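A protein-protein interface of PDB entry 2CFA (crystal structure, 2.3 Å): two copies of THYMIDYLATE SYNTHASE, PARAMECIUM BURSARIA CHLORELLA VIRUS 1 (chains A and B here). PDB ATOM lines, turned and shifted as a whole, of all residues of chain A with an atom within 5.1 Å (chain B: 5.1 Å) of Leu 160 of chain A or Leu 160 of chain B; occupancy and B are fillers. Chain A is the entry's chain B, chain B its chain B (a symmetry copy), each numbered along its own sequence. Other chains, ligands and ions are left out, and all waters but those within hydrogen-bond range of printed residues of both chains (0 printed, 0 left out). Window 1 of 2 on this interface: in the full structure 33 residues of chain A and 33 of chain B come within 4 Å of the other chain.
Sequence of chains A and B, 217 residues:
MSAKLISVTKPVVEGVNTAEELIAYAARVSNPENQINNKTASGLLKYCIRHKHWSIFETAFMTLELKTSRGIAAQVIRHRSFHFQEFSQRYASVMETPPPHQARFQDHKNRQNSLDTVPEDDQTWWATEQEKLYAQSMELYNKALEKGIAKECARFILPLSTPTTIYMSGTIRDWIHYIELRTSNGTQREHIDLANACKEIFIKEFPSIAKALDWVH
The backbone NH of Leu 160 of chain B sits at hydrogen-bond distance from the backbone carbonyl oxygen of Phe 156 of chain A, at 3.0 Å. The backbone carbonyl oxygen (O) of Phe 156 of chain A sits at hydrogen-bond distance from the backbone NH (N) of Ser 161 of chain B, at 2.9 Å. The backbone carbonyl oxygen (O) of Leu 158 of chain A lies within hydrogen-bond range of the backbone NH (N) of Leu 160 of chain B (3.0 Å). The backbone NH (N) of Leu 160 of chain A sits at hydrogen-bond distance from the backbone carbonyl oxygen (O) of Phe 156 of chain B (3.0 Å). N of Leu 160 of chain A is in hydrogen-bond range of O of Leu 158 of chain B (3.0 Å). O of Phe 156 of chain B sits at hydrogen-bond distance from N of Ser 161 of chain A (2.9 Å).
The backbone carbonyl oxygen of Leu 160 of chain A lies within hydrogen-bond range of the backbone NH of Arg 70 of chain A (3.2 Å). N of Arg 70 of chain A lies within hydrogen-bond range of O of Thr 162 of chain A, 2.9 Å away. The backbone carbonyl oxygen (O) of Leu 160 of chain A is in hydrogen-bond range of the backbone NH (N) of Gly 71 of chain A, at 2.9 Å. The backbone carbonyl oxygen of Pro 159 of chain A sits at hydrogen-bond distance from the side-chain hydroxyl of Thr 162 of chain A, at 2.5 Å. N of Gly 71 of chain B sits at hydrogen-bond distance from O of Leu 160 of chain B (2.9 Å). The side-chain hydroxyl (OG1) of Thr 162 of chain B lies within hydrogen-bond range of the backbone carbonyl oxygen (O) of Pro 159 of chain B, at 2.5 Å.
Among the printed residues, 21 pairs touch across the chains.
Of the printed residues of chain B, Ser 69 of chain A touches Phe 156. Leu 160 of chain A touches just these residues of chain B: Arg 70 (3.5 Å), Arg 155 (3.7 Å), Phe 156 (3.0 Å), Leu 158 (3.0 Å) and Leu 160 (3.6 Å). Thr 162 of chain A touches none of the printed residues of chain B. Printed residues of chain A within 4 Å of Gly 71 of chain B: Phe 156. Leu 160 of chain B touches just these residues of chain A: Arg 70, Arg 155, Phe 156, Leu 158 and Leu 160. Of the printed residues of chain A, Ser 161 of chain B touches Phe 156. Thr 162 of chain B touches none of the printed residues of chain A. The nearest residue of chain B that does not touch Leu 160 of chain A is Pro 159 of chain B (4.3 Å). The nearest printed residue of chain B that does not touch Phe 156 of chain A is Thr 162 of chain B (5.4 Å).
Ser 69 of chain A touches Phe 156 of chain B, and with the chains exchanged Phe 156 of chain A touches Ser 69 of chain B. Arg 70 of chain A touches Leu 160 of chain B, and with the chains exchanged Leu 160 of chain A touches Arg 70 of chain B. Ile 157 of chain A touches Pro 159 of chain B, and with the chains exchanged Pro 159 of chain A touches Ile 157 of chain B. Leu 158 of chain A touches Pro 159 of chain B, and with the chains exchanged Pro 159 of chain A touches Leu 158 of chain B. Of the 21 pairs that touch across the chains among the printed residues, 21 have their exchanged pair printed and touching as well.
Among the printed residues, merely in contact across the chains: Ser 69 of chain A with Phe 156 of chain B (3.3 Å), Arg 70 of chain A with Leu 160 of chain B (3.5 Å), Gly 71 of chain A with Phe 156 of chain B (3.996 Å), Arg 155 of chain A with Leu 160 of chain B (3.7 Å), Phe 156 of chain A with Ser 69 of chain B (3.3 Å), Phe 156 of chain A with Gly 71 of chain B (3.99 Å), Phe 156 of chain A with Pro 159 of chain B (3.7 Å), Ile 157 of chain A with Pro 159 of chain B (3.8 Å), Leu 158 of chain A with Pro 159 of chain B (3.3 Å), Pro 159 of chain A with Phe 156 of chain B (3.7 Å), Pro 159 of chain A with Ile 157 of chain B (3.8 Å), Pro 159 of chain A with Leu 158 of chain B (3.3 Å), Leu 160 of chain A with Arg 70 of chain B (3.5 Å), Leu 160 of chain A with Arg 155 of chain B (3.7 Å) and Leu 160 of chain A with Leu 160 of chain B (3.6 Å).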
ATOM      1  N   SER A  69       2.089 -30.336 -18.403  1.00  0.00           N
ATOM      2  CA  SER A  69       0.907 -29.906 -17.661  1.00  0.00           C
ATOM      3  C   SER A  69      -0.173 -30.987 -17.633  1.00  0.00           C
ATOM      4  O   SER A  69      -0.040 -32.025 -18.287  1.00  0.00           O
ATOM      5  CB  SER A  69       0.361 -28.592 -18.233  1.00  0.00           C
ATOM      6  OG  SER A  69       0.148 -28.683 -19.628  1.00  0.00           O
ATOM      7  N   ARG A  70      -1.235 -30.742 -16.869  1.00  0.00           N
ATOM      8  CA  ARG A  70      -2.385 -31.643 -16.817  1.00  0.00           C
ATOM      9  C   ARG A  70      -3.179 -31.663 -18.119  1.00  0.00           C
ATOM     10  O   ARG A  70      -3.813 -32.668 -18.442  1.00  0.00           O
ATOM     11  CB  ARG A  70      -3.308 -31.305 -15.636  1.00  0.00           C
ATOM     12  CG  ARG A  70      -2.700 -31.588 -14.268  1.00  0.00           C
ATOM     13  CD  ARG A  70      -2.583 -33.090 -13.989  1.00  0.00           C
ATOM     14  NE  ARG A  70      -3.694 -33.601 -13.186  1.00  0.00           N
ATOM     15  CZ  ARG A  70      -3.700 -33.624 -11.854  1.00  0.00           C
ATOM     16  NH1 ARG A  70      -2.654 -33.159 -11.176  1.00  0.00           N
ATOM     17  NH2 ARG A  70      -4.753 -34.104 -11.196  1.00  0.00           N
ATOM     18  N   GLY A  71      -3.146 -30.554 -18.853  1.00  0.00           N
ATOM     19  CA  GLY A  71      -3.806 -30.461 -20.162  1.00  0.00           C
ATOM     20  C   GLY A  71      -3.150 -31.354 -21.205  1.00  0.00           C
ATOM     21  O   GLY A  71      -3.833 -32.074 -21.940  1.00  0.00           O
ATOM     22  N   ARG A 155      -7.845 -31.009  -5.199  1.00  0.00           N
ATOM     23  CA  ARG A 155      -7.286 -31.208  -6.539  1.00  0.00           C
ATOM     24  C   ARG A 155      -8.158 -30.664  -7.670  1.00  0.00           C
ATOM     25  O   ARG A 155      -7.642 -30.134  -8.651  1.00  0.00           O
ATOM     26  CB  ARG A 155      -7.051 -32.702  -6.776  1.00  0.00           C
ATOM     27  CG  ARG A 155      -5.596 -33.113  -6.941  1.00  0.00           C
ATOM     28  CD  ARG A 155      -5.406 -34.634  -6.816  1.00  0.00           C
ATOM     29  NE  ARG A 155      -6.650 -35.403  -6.969  1.00  0.00           N
ATOM     30  CZ  ARG A 155      -7.108 -35.907  -8.115  1.00  0.00           C
ATOM     31  NH1 ARG A 155      -8.249 -36.587  -8.119  1.00  0.00           N
ATOM     32  NH2 ARG A 155      -6.441 -35.737  -9.253  1.00  0.00           N
ATOM     33  N   PHE A 156      -9.472 -30.799  -7.516  1.00  0.00           N
ATOM     34  CA  PHE A 156     -10.437 -30.469  -8.567  1.00  0.00           C
ATOM     35  C   PHE A 156     -10.509 -28.994  -8.966  1.00  0.00           C
ATOM     36  O   PHE A 156     -10.955 -28.671 -10.070  1.00  0.00           O
ATOM     37  CB  PHE A 156     -11.821 -31.010  -8.194  1.00  0.00           C
ATOM     38  CG  PHE A 156     -12.021 -32.456  -8.565  1.00  0.00           C
ATOM     39  CD1 PHE A 156     -12.944 -32.813  -9.541  1.00  0.00           C
ATOM     40  CD2 PHE A 156     -11.270 -33.457  -7.956  1.00  0.00           C
ATOM     41  CE1 PHE A 156     -13.126 -34.144  -9.898  1.00  0.00           C
ATOM     42  CE2 PHE A 156     -11.444 -34.793  -8.304  1.00  0.00           C
ATOM     43  CZ  PHE A 156     -12.375 -35.136  -9.279  1.00  0.00           C
ATOM     44  N   ILE A 157     -10.059 -28.110  -8.077  1.00  0.00           N
ATOM     45  CA  ILE A 157     -10.044 -26.668  -8.348  1.00  0.00           C
ATOM     46  C   ILE A 157      -8.791 -26.219  -9.107  1.00  0.00           C
ATOM     47  O   ILE A 157      -8.710 -25.078  -9.561  1.00  0.00           O
ATOM     48  CB  ILE A 157     -10.222 -25.826  -7.050  1.00  0.00           C
ATOM     49  CG1 ILE A 157      -8.983 -25.933  -6.148  1.00  0.00           C
ATOM     50  CG2 ILE A 157     -11.504 -26.235  -6.322  1.00  0.00           C
ATOM     51  CD1 ILE A 157      -8.913 -24.906  -5.028  1.00  0.00           C
ATOM     52  N   LEU A 158      -7.823 -27.122  -9.244  1.00  0.00           N
ATOM     53  CA  LEU A 158      -6.589 -26.831  -9.976  1.00  0.00           C
ATOM     54  C   LEU A 158      -6.844 -26.706 -11.479  1.00  0.00           C
ATOM     55  O   LEU A 158      -7.650 -27.454 -12.031  1.00  0.00           O
ATOM     56  CB  LEU A 158      -5.526 -27.898  -9.687  1.00  0.00           C
ATOM     57  CG  LEU A 158      -4.488 -27.671  -8.575  1.00  0.00           C
ATOM     58  CD1 LEU A 158      -4.921 -26.638  -7.528  1.00  0.00           C
ATOM     59  CD2 LEU A 158      -4.115 -28.993  -7.909  1.00  0.00           C
ATOM     60  N   PRO A 159      -6.170 -25.742 -12.141  1.00  0.00           N
ATOM     61  CA  PRO A 159      -6.306 -25.572 -13.586  1.00  0.00           C
ATOM     62  C   PRO A 159      -5.576 -26.659 -14.384  1.00  0.00           C
ATOM     63  O   PRO A 159      -4.751 -27.385 -13.832  1.00  0.00           O
ATOM     64  CB  PRO A 159      -5.649 -24.212 -13.832  1.00  0.00           C
ATOM     65  CG  PRO A 159      -4.624 -24.113 -12.773  1.00  0.00           C
ATOM     66  CD  PRO A 159      -5.248 -24.744 -11.563  1.00  0.00           C
ATOM     67  N   LEU A 160      -5.874 -26.749 -15.679  1.00  0.00           N
ATOM     68  CA  LEU A 160      -5.192 -27.684 -16.579  1.00  0.00           C
ATOM     69  C   LEU A 160      -3.735 -27.303 -16.819  1.00  0.00           C
ATOM     70  O   LEU A 160      -2.958 -28.107 -17.340  1.00  0.00           O
ATOM     71  CB  LEU A 160      -5.933 -27.781 -17.913  1.00  0.00           C
ATOM     72  CG  LEU A 160      -6.924 -28.923 -18.169  1.00  0.00           C
ATOM     73  CD1 LEU A 160      -7.870 -29.181 -17.003  1.00  0.00           C
ATOM     74  CD2 LEU A 160      -7.707 -28.626 -19.437  1.00  0.00           C
ATOM     75  N   SER A 161      -3.373 -26.079 -16.435  1.00  0.00           N
ATOM     76  CA  SER A 161      -2.004 -25.576 -16.571  1.00  0.00           C
ATOM     77  C   SER A 161      -1.088 -26.085 -15.458  1.00  0.00           C
ATOM     78  O   SER A 161       0.132 -25.919 -15.529  1.00  0.00           O
ATOM     79  CB  SER A 161      -1.989 -24.041 -16.617  1.00  0.00           C
ATOM     80  OG  SER A 161      -2.577 -23.476 -15.453  1.00  0.00           O
ATOM     81  N   THR A 162      -1.683 -26.696 -14.435  1.00  0.00           N
ATOM     82  CA  THR A 162      -0.945 -27.312 -13.331  1.00  0.00           C
ATOM     83  C   THR A 162       0.092 -28.326 -13.833  1.00  0.00           C
ATOM     84  O   THR A 162      -0.266 -29.275 -14.524  1.00  0.00           O
ATOM     85  CB  THR A 162      -1.908 -28.046 -12.380  1.00  0.00           C
ATOM     86  OG1 THR A 162      -3.009 -27.192 -12.058  1.00  0.00           O
ATOM     87  CG2 THR A 162      -1.197 -28.479 -11.095  1.00  0.00           C
ATOM     88  N   SER B  69     -16.711 -34.856 -14.811  1.00  0.00           N
ATOM     89  CA  SER B  69     -15.764 -33.745 -14.839  1.00  0.00           C
ATOM     90  C   SER B  69     -14.462 -34.126 -15.543  1.00  0.00           C
ATOM     91  O   SER B  69     -14.261 -35.287 -15.908  1.00  0.00           O
ATOM     92  CB  SER B  69     -15.496 -33.229 -13.419  1.00  0.00           C
ATOM     93  OG  SER B  69     -15.109 -34.278 -12.552  1.00  0.00           O
ATOM     94  N   ARG B  70     -13.586 -33.142 -15.738  1.00  0.00           N
ATOM     95  CA  ARG B  70     -12.263 -33.376 -16.317  1.00  0.00           C
ATOM     96  C   ARG B  70     -11.347 -34.168 -15.390  1.00  0.00           C
ATOM     97  O   ARG B  70     -10.453 -34.874 -15.859  1.00  0.00           O
ATOM     98  CB  ARG B  70     -11.593 -32.057 -16.730  1.00  0.00           C
ATOM     99  CG  ARG B  70     -12.264 -31.357 -17.905  1.00  0.00           C
ATOM    100  CD  ARG B  70     -12.039 -32.102 -19.224  1.00  0.00           C
ATOM    101  NE  ARG B  70     -10.935 -31.544 -20.006  1.00  0.00           N
ATOM    102  CZ  ARG B  70     -11.075 -30.560 -20.892  1.00  0.00           C
ATOM    103  NH1 ARG B  70     -12.274 -30.023 -21.106  1.00  0.00           N
ATOM    104  NH2 ARG B  70     -10.019 -30.105 -21.562  1.00  0.00           N
ATOM    105  N   GLY B  71     -11.567 -34.041 -14.084  1.00  0.00           N
ATOM    106  CA  GLY B  71     -10.806 -34.802 -13.083  1.00  0.00           C
ATOM    107  C   GLY B  71     -11.100 -36.294 -13.145  1.00  0.00           C
ATOM    108  O   GLY B  71     -10.181 -37.120 -13.127  1.00  0.00           O
ATOM    109  N   ARG B 155      -8.484 -22.950 -22.813  1.00  0.00           N
ATOM    110  CA  ARG B 155      -8.821 -24.213 -22.149  1.00  0.00           C
ATOM    111  C   ARG B 155      -7.987 -24.510 -20.905  1.00  0.00           C
ATOM    112  O   ARG B 155      -8.502 -25.044 -19.926  1.00  0.00           O
ATOM    113  CB  ARG B 155      -8.653 -25.368 -23.140  1.00  0.00           C
ATOM    114  CG  ARG B 155      -9.934 -26.103 -23.505  1.00  0.00           C
ATOM    115  CD  ARG B 155      -9.758 -26.993 -24.746  1.00  0.00           C
ATOM    116  NE  ARG B 155      -8.355 -27.276 -25.080  1.00  0.00           N
ATOM    117  CZ  ARG B 155      -7.659 -28.332 -24.657  1.00  0.00           C
ATOM    118  NH1 ARG B 155      -6.394 -28.473 -25.034  1.00  0.00           N
ATOM    119  NH2 ARG B 155      -8.214 -29.242 -23.862  1.00  0.00           N
ATOM    120  N   PHE B 156      -6.706 -24.156 -20.957  1.00  0.00           N
ATOM    121  CA  PHE B 156      -5.739 -24.502 -19.913  1.00  0.00           C
ATOM    122  C   PHE B 156      -5.986 -23.874 -18.540  1.00  0.00           C
ATOM    123  O   PHE B 156      -5.511 -24.391 -17.526  1.00  0.00           O
ATOM    124  CB  PHE B 156      -4.315 -24.216 -20.405  1.00  0.00           C
ATOM    125  CG  PHE B 156      -3.726 -25.336 -21.222  1.00  0.00           C
ATOM    126  CD1 PHE B 156      -2.639 -26.059 -20.746  1.00  0.00           C
ATOM    127  CD2 PHE B 156      -4.273 -25.681 -22.455  1.00  0.00           C
ATOM    128  CE1 PHE B 156      -2.096 -27.102 -21.488  1.00  0.00           C
ATOM    129  CE2 PHE B 156      -3.737 -26.722 -23.206  1.00  0.00           C
ATOM    130  CZ  PHE B 156      -2.646 -27.434 -22.721  1.00  0.00           C
ATOM    131  N   ILE B 157      -6.737 -22.774 -18.511  1.00  0.00           N
ATOM    132  CA  ILE B 157      -7.075 -22.091 -17.257  1.00  0.00           C
ATOM    133  C   ILE B 157      -8.306 -22.691 -16.567  1.00  0.00           C
ATOM    134  O   ILE B 157      -8.613 -22.347 -15.426  1.00  0.00           O
ATOM    135  CB  ILE B 157      -7.258 -20.558 -17.455  1.00  0.00           C
ATOM    136  CG1 ILE B 157      -8.528 -20.254 -18.265  1.00  0.00           C
ATOM    137  CG2 ILE B 157      -6.007 -19.950 -18.091  1.00  0.00           C
ATOM    138  CD1 ILE B 157      -8.974 -18.800 -18.236  1.00  0.00           C
ATOM    139  N   LEU B 158      -9.000 -23.588 -17.263  1.00  0.00           N
ATOM    140  CA  LEU B 158     -10.177 -24.259 -16.707  1.00  0.00           C
ATOM    141  C   LEU B 158      -9.791 -25.244 -15.603  1.00  0.00           C
ATOM    142  O   LEU B 158      -8.768 -25.920 -15.711  1.00  0.00           O
ATOM    143  CB  LEU B 158     -10.970 -24.962 -17.816  1.00  0.00           C
ATOM    144  CG  LEU B 158     -12.152 -24.244 -18.490  1.00  0.00           C
ATOM    145  CD1 LEU B 158     -12.108 -22.718 -18.353  1.00  0.00           C
ATOM    146  CD2 LEU B 158     -12.262 -24.653 -19.958  1.00  0.00           C
ATOM    147  N   PRO B 159     -10.601 -25.311 -14.526  1.00  0.00           N
ATOM    148  CA  PRO B 159     -10.348 -26.255 -13.438  1.00  0.00           C
ATOM    149  C   PRO B 159     -10.693 -27.701 -13.814  1.00  0.00           C
ATOM    150  O   PRO B 159     -11.371 -27.937 -14.811  1.00  0.00           O
ATOM    151  CB  PRO B 159     -11.286 -25.762 -12.335  1.00  0.00           C
ATOM    152  CG  PRO B 159     -12.417 -25.160 -13.070  1.00  0.00           C
ATOM    153  CD  PRO B 159     -11.799 -24.490 -14.261  1.00  0.00           C
ATOM    154  N   LEU B 160     -10.237 -28.652 -13.000  1.00  0.00           N
ATOM    155  CA  LEU B 160     -10.561 -30.069 -13.189  1.00  0.00           C
ATOM    156  C   LEU B 160     -12.030 -30.372 -12.914  1.00  0.00           C
ATOM    157  O   LEU B 160     -12.521 -31.448 -13.263  1.00  0.00           O
ATOM    158  CB  LEU B 160      -9.672 -30.945 -12.307  1.00  0.00           C
ATOM    159  CG  LEU B 160      -8.409 -31.597 -12.881  1.00  0.00           C
ATOM    160  CD1 LEU B 160      -7.567 -30.651 -13.728  1.00  0.00           C
ATOM    161  CD2 LEU B 160      -7.583 -32.170 -11.741  1.00  0.00           C
ATOM    162  N   SER B 161     -12.723 -29.419 -12.290  1.00  0.00           N
ATOM    163  CA  SER B 161     -14.148 -29.547 -11.980  1.00  0.00           C
ATOM    164  C   SER B 161     -15.032 -29.253 -13.193  1.00  0.00           C
ATOM    165  O   SER B 161     -16.239 -29.503 -13.161  1.00  0.00           O
ATOM    166  CB  SER B 161     -14.535 -28.639 -10.803  1.00  0.00           C
ATOM    167  OG  SER B 161     -14.240 -27.276 -11.073  1.00  0.00           O
ATOM    168  N   THR B 162     -14.425 -28.717 -14.250  1.00  0.00           N
ATOM    169  CA  THR B 162     -15.110 -28.452 -15.516  1.00  0.00           C
ATOM    170  C   THR B 162     -15.802 -29.707 -16.065  1.00  0.00           C
ATOM    171  O   THR B 162     -15.146 -30.721 -16.283  1.00  0.00           O
ATOM    172  CB  THR B 162     -14.111 -27.957 -16.578  1.00  0.00           C
ATOM    173  OG1 THR B 162     -13.297 -26.918 -16.024  1.00  0.00           O
ATOM    174  CG2 THR B 162     -14.836 -27.436 -17.822  1.00  0.00           C
